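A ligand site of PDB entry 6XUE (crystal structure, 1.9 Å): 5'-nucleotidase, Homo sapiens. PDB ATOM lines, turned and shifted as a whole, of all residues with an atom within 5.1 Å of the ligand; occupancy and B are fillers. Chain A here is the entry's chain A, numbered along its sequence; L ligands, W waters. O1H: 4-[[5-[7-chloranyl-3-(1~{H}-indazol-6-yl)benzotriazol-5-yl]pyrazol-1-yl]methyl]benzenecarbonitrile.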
ATOM      1  N   ASN A  91       1.482 -37.155  26.221  1.00  0.00           N
ATOM      2  CA  ASN A  91       0.751 -36.008  26.765  1.00  0.00           C
ATOM      3  C   ASN A  91       0.051 -35.192  25.672  1.00  0.00           C
ATOM      4  O   ASN A  91      -1.112 -34.846  25.881  1.00  0.00           O
ATOM      5  CB  ASN A  91       1.637 -35.091  27.626  1.00  0.00           C
ATOM      6  CG  ASN A  91       2.949 -34.686  27.017  1.00  0.00           C
ATOM      7  OD1 ASN A  91       3.862 -35.492  26.880  1.00  0.00           O
ATOM      8  ND2 ASN A  91       3.082 -33.394  26.659  1.00  0.00           N
ATOM      9  N   HIS A  92       0.697 -34.986  24.499  1.00  0.00           N
ATOM     10  CA  HIS A  92       0.120 -34.197  23.390  1.00  0.00           C
ATOM     11  C   HIS A  92      -1.124 -34.851  22.741  1.00  0.00           C
ATOM     12  O   HIS A  92      -1.913 -34.112  22.148  1.00  0.00           O
ATOM     13  CB  HIS A  92       1.170 -33.797  22.359  1.00  0.00           C
ATOM     14  CG  HIS A  92       2.052 -32.661  22.815  1.00  0.00           C
ATOM     15  ND1 HIS A  92       1.635 -31.345  22.735  1.00  0.00           N
ATOM     16  CD2 HIS A  92       3.290 -32.693  23.379  1.00  0.00           C
ATOM     17  CE1 HIS A  92       2.628 -30.610  23.239  1.00  0.00           C
ATOM     18  NE2 HIS A  92       3.644 -31.376  23.634  1.00  0.00           N
ATOM     19  N   PHE A  94      -3.699 -35.562  24.203  1.00  0.00           N
ATOM     20  CA  PHE A  94      -4.797 -34.972  24.983  1.00  0.00           C
ATOM     21  C   PHE A  94      -4.987 -33.461  24.727  1.00  0.00           C
ATOM     22  O   PHE A  94      -5.838 -32.863  25.373  1.00  0.00           O
ATOM     23  CB  PHE A  94      -4.622 -35.229  26.497  1.00  0.00           C
ATOM     24  CG  PHE A  94      -4.662 -36.694  26.861  1.00  0.00           C
ATOM     25  CD1 PHE A  94      -5.879 -37.316  27.099  1.00  0.00           C
ATOM     26  CD2 PHE A  94      -3.498 -37.446  26.918  1.00  0.00           C
ATOM     27  CE1 PHE A  94      -5.924 -38.685  27.402  1.00  0.00           C
ATOM     28  CE2 PHE A  94      -3.550 -38.815  27.229  1.00  0.00           C
ATOM     29  CZ  PHE A  94      -4.757 -39.418  27.463  1.00  0.00           C
ATOM     30  N   ASP A  95      -4.176 -32.859  23.812  1.00  0.00           N
ATOM     31  CA  ASP A  95      -4.226 -31.413  23.512  1.00  0.00           C
ATOM     32  C   ASP A  95      -5.593 -30.862  23.089  1.00  0.00           C
ATOM     33  O   ASP A  95      -5.904 -29.705  23.393  1.00  0.00           O
ATOM     34  CB  ASP A  95      -3.166 -31.042  22.461  1.00  0.00           C
ATOM     35  CG  ASP A  95      -1.768 -30.887  22.996  1.00  0.00           C
ATOM     36  OD1 ASP A  95      -1.554 -31.132  24.219  1.00  0.00           O
ATOM     37  OD2 ASP A  95      -0.871 -30.491  22.210  1.00  0.00           O
ATOM     38  N   PRO A 156      -1.770 -33.928  33.272  1.00  0.00           N
ATOM     39  CA  PRO A 156      -2.714 -32.829  33.618  1.00  0.00           C
ATOM     40  C   PRO A 156      -2.118 -31.407  33.665  1.00  0.00           C
ATOM     41  O   PRO A 156      -2.873 -30.438  33.480  1.00  0.00           O
ATOM     42  CB  PRO A 156      -3.229 -33.227  35.011  1.00  0.00           C
ATOM     43  CG  PRO A 156      -3.087 -34.736  35.042  1.00  0.00           C
ATOM     44  CD  PRO A 156      -1.790 -34.986  34.310  1.00  0.00           C
ATOM     45  N   PHE A 157      -0.786 -31.275  33.912  1.00  0.00           N
ATOM     46  CA  PHE A 157      -0.144 -29.960  33.990  1.00  0.00           C
ATOM     47  C   PHE A 157       0.413 -29.524  32.628  1.00  0.00           C
ATOM     48  O   PHE A 157       0.882 -28.394  32.489  1.00  0.00           O
ATOM     49  CB  PHE A 157       0.937 -29.961  35.088  1.00  0.00           C
ATOM     50  CG  PHE A 157       0.372 -30.232  36.461  1.00  0.00           C
ATOM     51  CD1 PHE A 157      -0.150 -29.198  37.236  1.00  0.00           C
ATOM     52  CD2 PHE A 157       0.287 -31.530  36.957  1.00  0.00           C
ATOM     53  CE1 PHE A 157      -0.705 -29.457  38.490  1.00  0.00           C
ATOM     54  CE2 PHE A 157      -0.282 -31.786  38.211  1.00  0.00           C
ATOM     55  CZ  PHE A 157      -0.773 -30.745  38.974  1.00  0.00           C
ATOM     56  N   LEU A 158       0.332 -30.443  31.627  1.00  0.00           N
ATOM     57  CA  LEU A 158       0.855 -30.208  30.266  1.00  0.00           C
ATOM     58  C   LEU A 158      -0.189 -30.199  29.150  1.00  0.00           C
ATOM     59  O   LEU A 158       0.098 -29.694  28.072  1.00  0.00           O
ATOM     60  CB  LEU A 158       1.952 -31.253  29.938  1.00  0.00           C
ATOM     61  CG  LEU A 158       3.072 -31.447  30.984  1.00  0.00           C
ATOM     62  CD1 LEU A 158       3.975 -32.584  30.608  1.00  0.00           C
ATOM     63  CD2 LEU A 158       3.860 -30.114  31.260  1.00  0.00           C
ATOM     64  N   SER A 159      -1.370 -30.776  29.384  1.00  0.00           N
ATOM     65  CA  SER A 159      -2.355 -30.933  28.324  1.00  0.00           C
ATOM     66  C   SER A 159      -3.814 -30.841  28.852  1.00  0.00           C
ATOM     67  O   SER A 159      -4.041 -30.303  29.938  1.00  0.00           O
ATOM     68  CB  SER A 159      -2.077 -32.258  27.603  1.00  0.00           C
ATOM     69  OG  SER A 159      -2.727 -32.347  26.346  1.00  0.00           O
ATOM     70  N   ASN A 160      -4.808 -31.379  28.091  1.00  0.00           N
ATOM     71  CA  ASN A 160      -6.197 -31.301  28.533  1.00  0.00           C
ATOM     72  C   ASN A 160      -6.876 -32.697  28.675  1.00  0.00           C
ATOM     73  O   ASN A 160      -7.881 -32.950  27.999  1.00  0.00           O
ATOM     74  CB  ASN A 160      -6.998 -30.349  27.614  1.00  0.00           C
ATOM     75  CG  ASN A 160      -8.409 -29.974  28.085  1.00  0.00           C
ATOM     76  OD1 ASN A 160      -8.779 -30.114  29.262  1.00  0.00           O
ATOM     77  ND2 ASN A 160      -9.215 -29.476  27.162  1.00  0.00           N
ATOM     78  N   HIS A 217       9.351 -38.508  25.107  1.00  0.00           N
ATOM     79  CA  HIS A 217       9.045 -37.302  25.925  1.00  0.00           C
ATOM     80  C   HIS A 217      10.224 -36.371  26.181  1.00  0.00           C
ATOM     81  O   HIS A 217      10.040 -35.153  26.141  1.00  0.00           O
ATOM     82  CB  HIS A 217       8.370 -37.673  27.267  1.00  0.00           C
ATOM     83  CG  HIS A 217       7.855 -36.514  28.082  1.00  0.00           C
ATOM     84  ND1 HIS A 217       6.869 -35.660  27.591  1.00  0.00           N
ATOM     85  CD2 HIS A 217       8.160 -36.131  29.347  1.00  0.00           C
ATOM     86  CE1 HIS A 217       6.634 -34.787  28.563  1.00  0.00           C
ATOM     87  NE2 HIS A 217       7.372 -35.037  29.640  1.00  0.00           N
ATOM     88  N   ARG A 328      15.109 -24.641  26.315  1.00  0.00           N
ATOM     89  CA  ARG A 328      14.868 -25.380  27.537  1.00  0.00           C
ATOM     90  C   ARG A 328      16.141 -25.440  28.414  1.00  0.00           C
ATOM     91  O   ARG A 328      16.095 -25.923  29.543  1.00  0.00           O
ATOM     92  CB  ARG A 328      14.291 -26.787  27.248  1.00  0.00           C
ATOM     93  CG  ARG A 328      12.848 -26.782  26.728  1.00  0.00           C
ATOM     94  CD  ARG A 328      12.255 -28.181  26.714  1.00  0.00           C
ATOM     95  NE  ARG A 328      10.949 -28.262  26.046  1.00  0.00           N
ATOM     96  CZ  ARG A 328      10.049 -29.221  26.258  1.00  0.00           C
ATOM     97  NH1 ARG A 328      10.258 -30.158  27.178  1.00  0.00           N
ATOM     98  NH2 ARG A 328       8.907 -29.223  25.576  1.00  0.00           N
ATOM     99  N   ASN A 364       7.615 -19.967  29.237  1.00  0.00           N
ATOM    100  CA  ASN A 364       8.146 -21.332  29.363  1.00  0.00           C
ATOM    101  C   ASN A 364       8.709 -21.843  28.022  1.00  0.00           C
ATOM    102  O   ASN A 364       8.083 -21.649  26.975  1.00  0.00           O
ATOM    103  CB  ASN A 364       7.070 -22.294  29.929  1.00  0.00           C
ATOM    104  CG  ASN A 364       5.839 -22.409  29.062  1.00  0.00           C
ATOM    105  OD1 ASN A 364       5.212 -21.415  28.707  1.00  0.00           O
ATOM    106  ND2 ASN A 364       5.464 -23.638  28.701  1.00  0.00           N
ATOM    107  N   GLY A 366       8.854 -24.799  27.037  1.00  0.00           N
ATOM    108  CA  GLY A 366       7.917 -25.833  26.584  1.00  0.00           C
ATOM    109  C   GLY A 366       6.800 -25.308  25.683  1.00  0.00           C
ATOM    110  O   GLY A 366       6.142 -26.104  25.007  1.00  0.00           O
ATOM    111  N   GLY A 367       6.606 -23.982  25.678  1.00  0.00           N
ATOM    112  CA  GLY A 367       5.654 -23.284  24.811  1.00  0.00           C
ATOM    113  C   GLY A 367       6.243 -22.868  23.468  1.00  0.00           C
ATOM    114  O   GLY A 367       5.501 -22.418  22.581  1.00  0.00           O
ATOM    115  N   ARG A 369       7.925 -24.154  20.215  1.00  0.00           N
ATOM    116  CA  ARG A 369       7.903 -25.476  19.569  1.00  0.00           C
ATOM    117  C   ARG A 369       8.718 -25.678  18.286  1.00  0.00           C
ATOM    118  O   ARG A 369       8.795 -26.829  17.836  1.00  0.00           O
ATOM    119  CB  ARG A 369       6.439 -25.885  19.320  1.00  0.00           C
ATOM    120  CG  ARG A 369       5.513 -25.701  20.530  1.00  0.00           C
ATOM    121  CD  ARG A 369       5.877 -26.556  21.732  1.00  0.00           C
ATOM    122  NE  ARG A 369       5.920 -27.987  21.413  1.00  0.00           N
ATOM    123  CZ  ARG A 369       6.090 -28.946  22.319  1.00  0.00           C
ATOM    124  NH1 ARG A 369       6.145 -30.220  21.931  1.00  0.00           N
ATOM    125  NH2 ARG A 369       6.194 -28.648  23.602  1.00  0.00           N
ATOM    126  N   PHE A 391      -0.684 -23.809  20.139  1.00  0.00           N
ATOM    127  CA  PHE A 391      -1.731 -24.150  21.132  1.00  0.00           C
ATOM    128  C   PHE A 391      -2.993 -23.293  21.150  1.00  0.00           C
ATOM    129  O   PHE A 391      -3.976 -23.693  21.773  1.00  0.00           O
ATOM    130  CB  PHE A 391      -1.134 -24.198  22.547  1.00  0.00           C
ATOM    131  CG  PHE A 391       0.023 -25.161  22.677  1.00  0.00           C
ATOM    132  CD1 PHE A 391      -0.201 -26.546  22.703  1.00  0.00           C
ATOM    133  CD2 PHE A 391       1.333 -24.701  22.707  1.00  0.00           C
ATOM    134  CE1 PHE A 391       0.876 -27.429  22.810  1.00  0.00           C
ATOM    135  CE2 PHE A 391       2.410 -25.591  22.798  1.00  0.00           C
ATOM    136  CZ  PHE A 391       2.174 -26.957  22.842  1.00  0.00           C
ATOM    137  N   GLY A 393      -3.435 -20.290  22.594  1.00  0.00           N
ATOM    138  CA  GLY A 393      -3.590 -19.654  23.904  1.00  0.00           C
ATOM    139  C   GLY A 393      -3.522 -18.138  23.818  1.00  0.00           C
ATOM    140  O   GLY A 393      -3.463 -17.581  22.719  1.00  0.00           O
ATOM    141  N   GLY A 421      10.077 -28.652  30.160  1.00  0.00           N
ATOM    142  CA  GLY A 421       9.563 -27.380  29.670  1.00  0.00           C
ATOM    143  C   GLY A 421       9.495 -26.157  30.567  1.00  0.00           C
ATOM    144  O   GLY A 421       9.289 -25.055  30.049  1.00  0.00           O
ATOM    145  N   PRO A 472       1.985 -16.325  29.383  1.00  0.00           N
ATOM    146  CA  PRO A 472       0.869 -17.068  28.764  1.00  0.00           C
ATOM    147  C   PRO A 472      -0.170 -17.492  29.806  1.00  0.00           C
ATOM    148  O   PRO A 472       0.170 -17.716  30.973  1.00  0.00           O
ATOM    149  CB  PRO A 472       1.552 -18.290  28.124  1.00  0.00           C
ATOM    150  CG  PRO A 472       3.024 -17.974  28.117  1.00  0.00           C
ATOM    151  CD  PRO A 472       3.239 -17.108  29.315  1.00  0.00           C
ATOM    152  N   PHE A 474      -1.512 -20.234  30.036  1.00  0.00           N
ATOM    153  CA  PHE A 474      -1.066 -21.576  30.423  1.00  0.00           C
ATOM    154  C   PHE A 474      -0.332 -21.542  31.780  1.00  0.00           C
ATOM    155  O   PHE A 474      -0.602 -22.386  32.633  1.00  0.00           O
ATOM    156  CB  PHE A 474      -0.158 -22.158  29.298  1.00  0.00           C
ATOM    157  CG  PHE A 474       0.567 -23.422  29.632  1.00  0.00           C
ATOM    158  CD1 PHE A 474      -0.096 -24.643  29.666  1.00  0.00           C
ATOM    159  CD2 PHE A 474       1.929 -23.414  29.906  1.00  0.00           C
ATOM    160  CE1 PHE A 474       0.579 -25.822  29.979  1.00  0.00           C
ATOM    161  CE2 PHE A 474       2.611 -24.593  30.213  1.00  0.00           C
ATOM    162  CZ  PHE A 474       1.936 -25.799  30.234  1.00  0.00           C
ATOM    163  N   ASN A 477      -2.520 -20.459  34.813  1.00  0.00           N
ATOM    164  CA  ASN A 477      -3.354 -21.620  35.147  1.00  0.00           C
ATOM    165  C   ASN A 477      -2.555 -22.811  35.722  1.00  0.00           C
ATOM    166  O   ASN A 477      -3.097 -23.905  35.843  1.00  0.00           O
ATOM    167  CB  ASN A 477      -4.202 -22.030  33.948  1.00  0.00           C
ATOM    168  CG  ASN A 477      -5.353 -21.077  33.664  1.00  0.00           C
ATOM    169  OD1 ASN A 477      -5.427 -20.454  32.602  1.00  0.00           O
ATOM    170  ND2 ASN A 477      -6.263 -20.946  34.613  1.00  0.00           N
ATOM    171  N   GLY A 478      -1.311 -22.560  36.112  1.00  0.00           N
ATOM    172  CA  GLY A 478      -0.443 -23.556  36.736  1.00  0.00           C
ATOM    173  C   GLY A 478       0.201 -24.593  35.828  1.00  0.00           C
ATOM    174  O   GLY A 478       0.702 -25.605  36.326  1.00  0.00           O
ATOM    175  N   GLY A 479       0.236 -24.319  34.520  1.00  0.00           N
ATOM    176  CA  GLY A 479       0.885 -25.199  33.549  1.00  0.00           C
ATOM    177  C   GLY A 479       2.371 -25.305  33.820  1.00  0.00           C
ATOM    178  O   GLY A 479       2.950 -24.385  34.416  1.00  0.00           O
ATOM    179  N   ASP A 480       2.985 -26.449  33.460  1.00  0.00           N
ATOM    180  CA  ASP A 480       4.418 -26.743  33.684  1.00  0.00           C
ATOM    181  C   ASP A 480       4.789 -26.860  35.162  1.00  0.00           C
ATOM    182  O   ASP A 480       5.969 -26.816  35.508  1.00  0.00           O
ATOM    183  CB  ASP A 480       5.357 -25.751  32.931  1.00  0.00           C
ATOM    184  CG  ASP A 480       5.948 -26.309  31.647  1.00  0.00           C
ATOM    185  OD1 ASP A 480       6.328 -27.507  31.634  1.00  0.00           O
ATOM    186  OD2 ASP A 480       6.037 -25.562  30.659  1.00  0.00           O
ATOM    187  N   ASP A 498      -2.040 -15.532  21.215  1.00  0.00           N
ATOM    188  CA  ASP A 498      -0.589 -15.685  21.143  1.00  0.00           C
ATOM    189  C   ASP A 498       0.042 -15.452  19.751  1.00  0.00           C
ATOM    190  O   ASP A 498       0.887 -14.562  19.623  1.00  0.00           O
ATOM    191  CB  ASP A 498      -0.109 -17.035  21.739  1.00  0.00           C
ATOM    192  CG  ASP A 498      -0.796 -18.332  21.309  1.00  0.00           C
ATOM    193  OD1 ASP A 498      -1.355 -18.383  20.193  1.00  0.00           O
ATOM    194  OD2 ASP A 498      -0.743 -19.308  22.091  1.00  0.00           O
HETATM  195  N1  O1H L   1      -3.465 -26.567  26.995  1.00  0.00           N
HETATM  196  N3  O1H L   1       2.467 -23.796  26.346  1.00  0.00           N
HETATM  197  C4  O1H L   1      -2.548 -27.969  25.578  1.00  0.00           C
HETATM  198  C5  O1H L   1      -3.847 -28.346  25.897  1.00  0.00           C
HETATM  199  C6  O1H L   1      -3.791 -25.512  27.963  1.00  0.00           C
HETATM  200  C7  O1H L   1      -3.464 -25.890  29.388  1.00  0.00           C
HETATM  201  C8  O1H L   1      -3.065 -27.176  29.741  1.00  0.00           C
HETATM  202  C10 O1H L   1      -2.853 -26.527  32.050  1.00  0.00           C
HETATM  203  C13 O1H L   1      -3.556 -24.934  30.397  1.00  0.00           C
HETATM  204  C15 O1H L   1       1.239 -25.685  26.563  1.00  0.00           C
HETATM  205  C17 O1H L   1       3.263 -27.148  27.070  1.00  0.00           C
HETATM  206  C20 O1H L   1       5.635 -30.503  27.900  1.00  0.00           C
HETATM  207  C21 O1H L   1       4.651 -29.545  27.502  1.00  0.00           C
HETATM  208  C22 O1H L   1       3.570 -29.493  26.609  1.00  0.00           C
HETATM  209  N2  O1H L   1      -2.182 -27.115  34.471  1.00  0.00           N
HETATM  210  C11 O1H L   1      -2.494 -26.845  33.408  1.00  0.00           C
HETATM  211  C9  O1H L   1      -2.765 -27.505  31.051  1.00  0.00           C
HETATM  212  C12 O1H L   1      -3.266 -25.241  31.711  1.00  0.00           C
HETATM  213  N   O1H L   1      -4.425 -27.516  26.753  1.00  0.00           N
HETATM  214  C3  O1H L   1      -2.322 -26.797  26.289  1.00  0.00           C
HETATM  215  C2  O1H L   1      -1.118 -25.942  26.292  1.00  0.00           C
HETATM  216  C1  O1H L   1      -1.206 -24.596  25.950  1.00  0.00           C
HETATM  217  C14 O1H L   1       0.120 -26.501  26.607  1.00  0.00           C
HETATM  218  N5  O1H L   1       2.566 -25.924  26.808  1.00  0.00           N
HETATM  219  N4  O1H L   1       3.277 -24.763  26.678  1.00  0.00           N
HETATM  220  C16 O1H L   1       1.204 -24.321  26.248  1.00  0.00           C
HETATM  221  C   O1H L   1      -0.063 -23.808  25.930  1.00  0.00           C
HETATM  222 CL   O1H L   1      -0.199 -22.157  25.401  1.00  0.00          CL
HETATM  223  C23 O1H L   1       2.894 -28.311  26.383  1.00  0.00           C
HETATM  224  C19 O1H L   1       5.024 -28.357  28.164  1.00  0.00           C
HETATM  225  C18 O1H L   1       4.336 -27.159  27.970  1.00  0.00           C
HETATM  226  N7  O1H L   1       6.522 -29.958  28.709  1.00  0.00           N
HETATM  227  N6  O1H L   1       6.136 -28.657  28.879  1.00  0.00           N
HETATM  228  O   HOH W   1       8.323 -30.932  30.639  1.00  0.00           O
HETATM  229  O   HOH W   2       0.053 -19.135  24.886  1.00  0.00           O
HETATM  230  O   HOH W   3       3.113 -21.102  27.009  1.00  0.00           O
HETATM  231  O   HOH W   4      -2.815 -26.463  37.649  1.00  0.00           O
HETATM  232  O   HOH W   5      -3.092 -21.836  27.329  1.00  0.00           O
HETATM  233  O   HOH W   6       0.831 -31.453  25.970  1.00  0.00           O
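A nitrogen (N6) of the ligand sits at hydrogen-bond distance from the side-chain carboxylate (OD1) of Asp 480 (3.0 Å).
N4 of the ligand lies within hydrogen-bond range of ND2 of Asn 364 (3.2 Å).
Residues that only touch the ligand: Ser 159 (3.3 Å), Gly 367 (3.4 Å), Phe 391 (3.4 Å), Phe 474 (3.5 Å), Leu 158 (3.5 Å), Asp 95 (3.5 Å), His 92 (3.5 Å), Phe 157 (3.5 Å), Pro 156 (3.5 Å), Gly 366 (3.6 Å), Asn 477 (3.6 Å), Gly 479 (3.7 Å), Gly 478 (3.7 Å), Gly 421 (3.7 Å), Asn 160 (3.9 Å) and Asn 91 (3.9 Å).
The nearest printed residue that does not touch the ligand is Arg 328 (4.01 Å).
Water W1 bridges a nitrogen (N7) of the ligand (2.8 Å) and the backbone NH of Gly 421 (2.9 Å).
Water W3 lies within hydrogen-bond range of OD1 of Asn 364 (2.7 Å) and N3 of the ligand (2.8 Å).
Water W4 bridges the backbone carbonyl oxygen (O) of Asn 477 (3.1 Å) and a nitrogen (N2) of the ligand (3.3 Å).
Water W6 lies within hydrogen-bond range of the backbone carbonyl oxygen of Leu 158 (2.8 Å), the side-chain carboxylate of Asp 95 (3.0 Å), the side-chain amide nitrogen of Asn 91 (3.1 Å) and a ring nitrogen (ND1) of His 92 (3.3 Å).
The side-chain amide nitrogen (ND2) of Asn 364 is in hydrogen-bond range of the side-chain carboxylate (OD2) of Asp 480 (2.8 Å).
N of Gly 367 sits close to ND2 of Asn 364 (3.2 Å).
OD1 of Asp 95 lies within hydrogen-bond range of OG of Ser 159 (2.7 Å).
O of Asn 91 lies within hydrogen-bond range of OG of Ser 159.
O of Phe 474 lies within hydrogen-bond range of N of Gly 479.
The side-chain carboxylate (OD2) of Asp 95 sits at hydrogen-bond distance from a ring nitrogen (ND1) of His 92, at 2.7 Å.
NE2 of His 92 lies within hydrogen-bond range of NH1 of Arg 369.
The backbone NH of Asn 160 lies within hydrogen-bond range of the backbone carbonyl oxygen of Phe 94 (3.3 Å).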
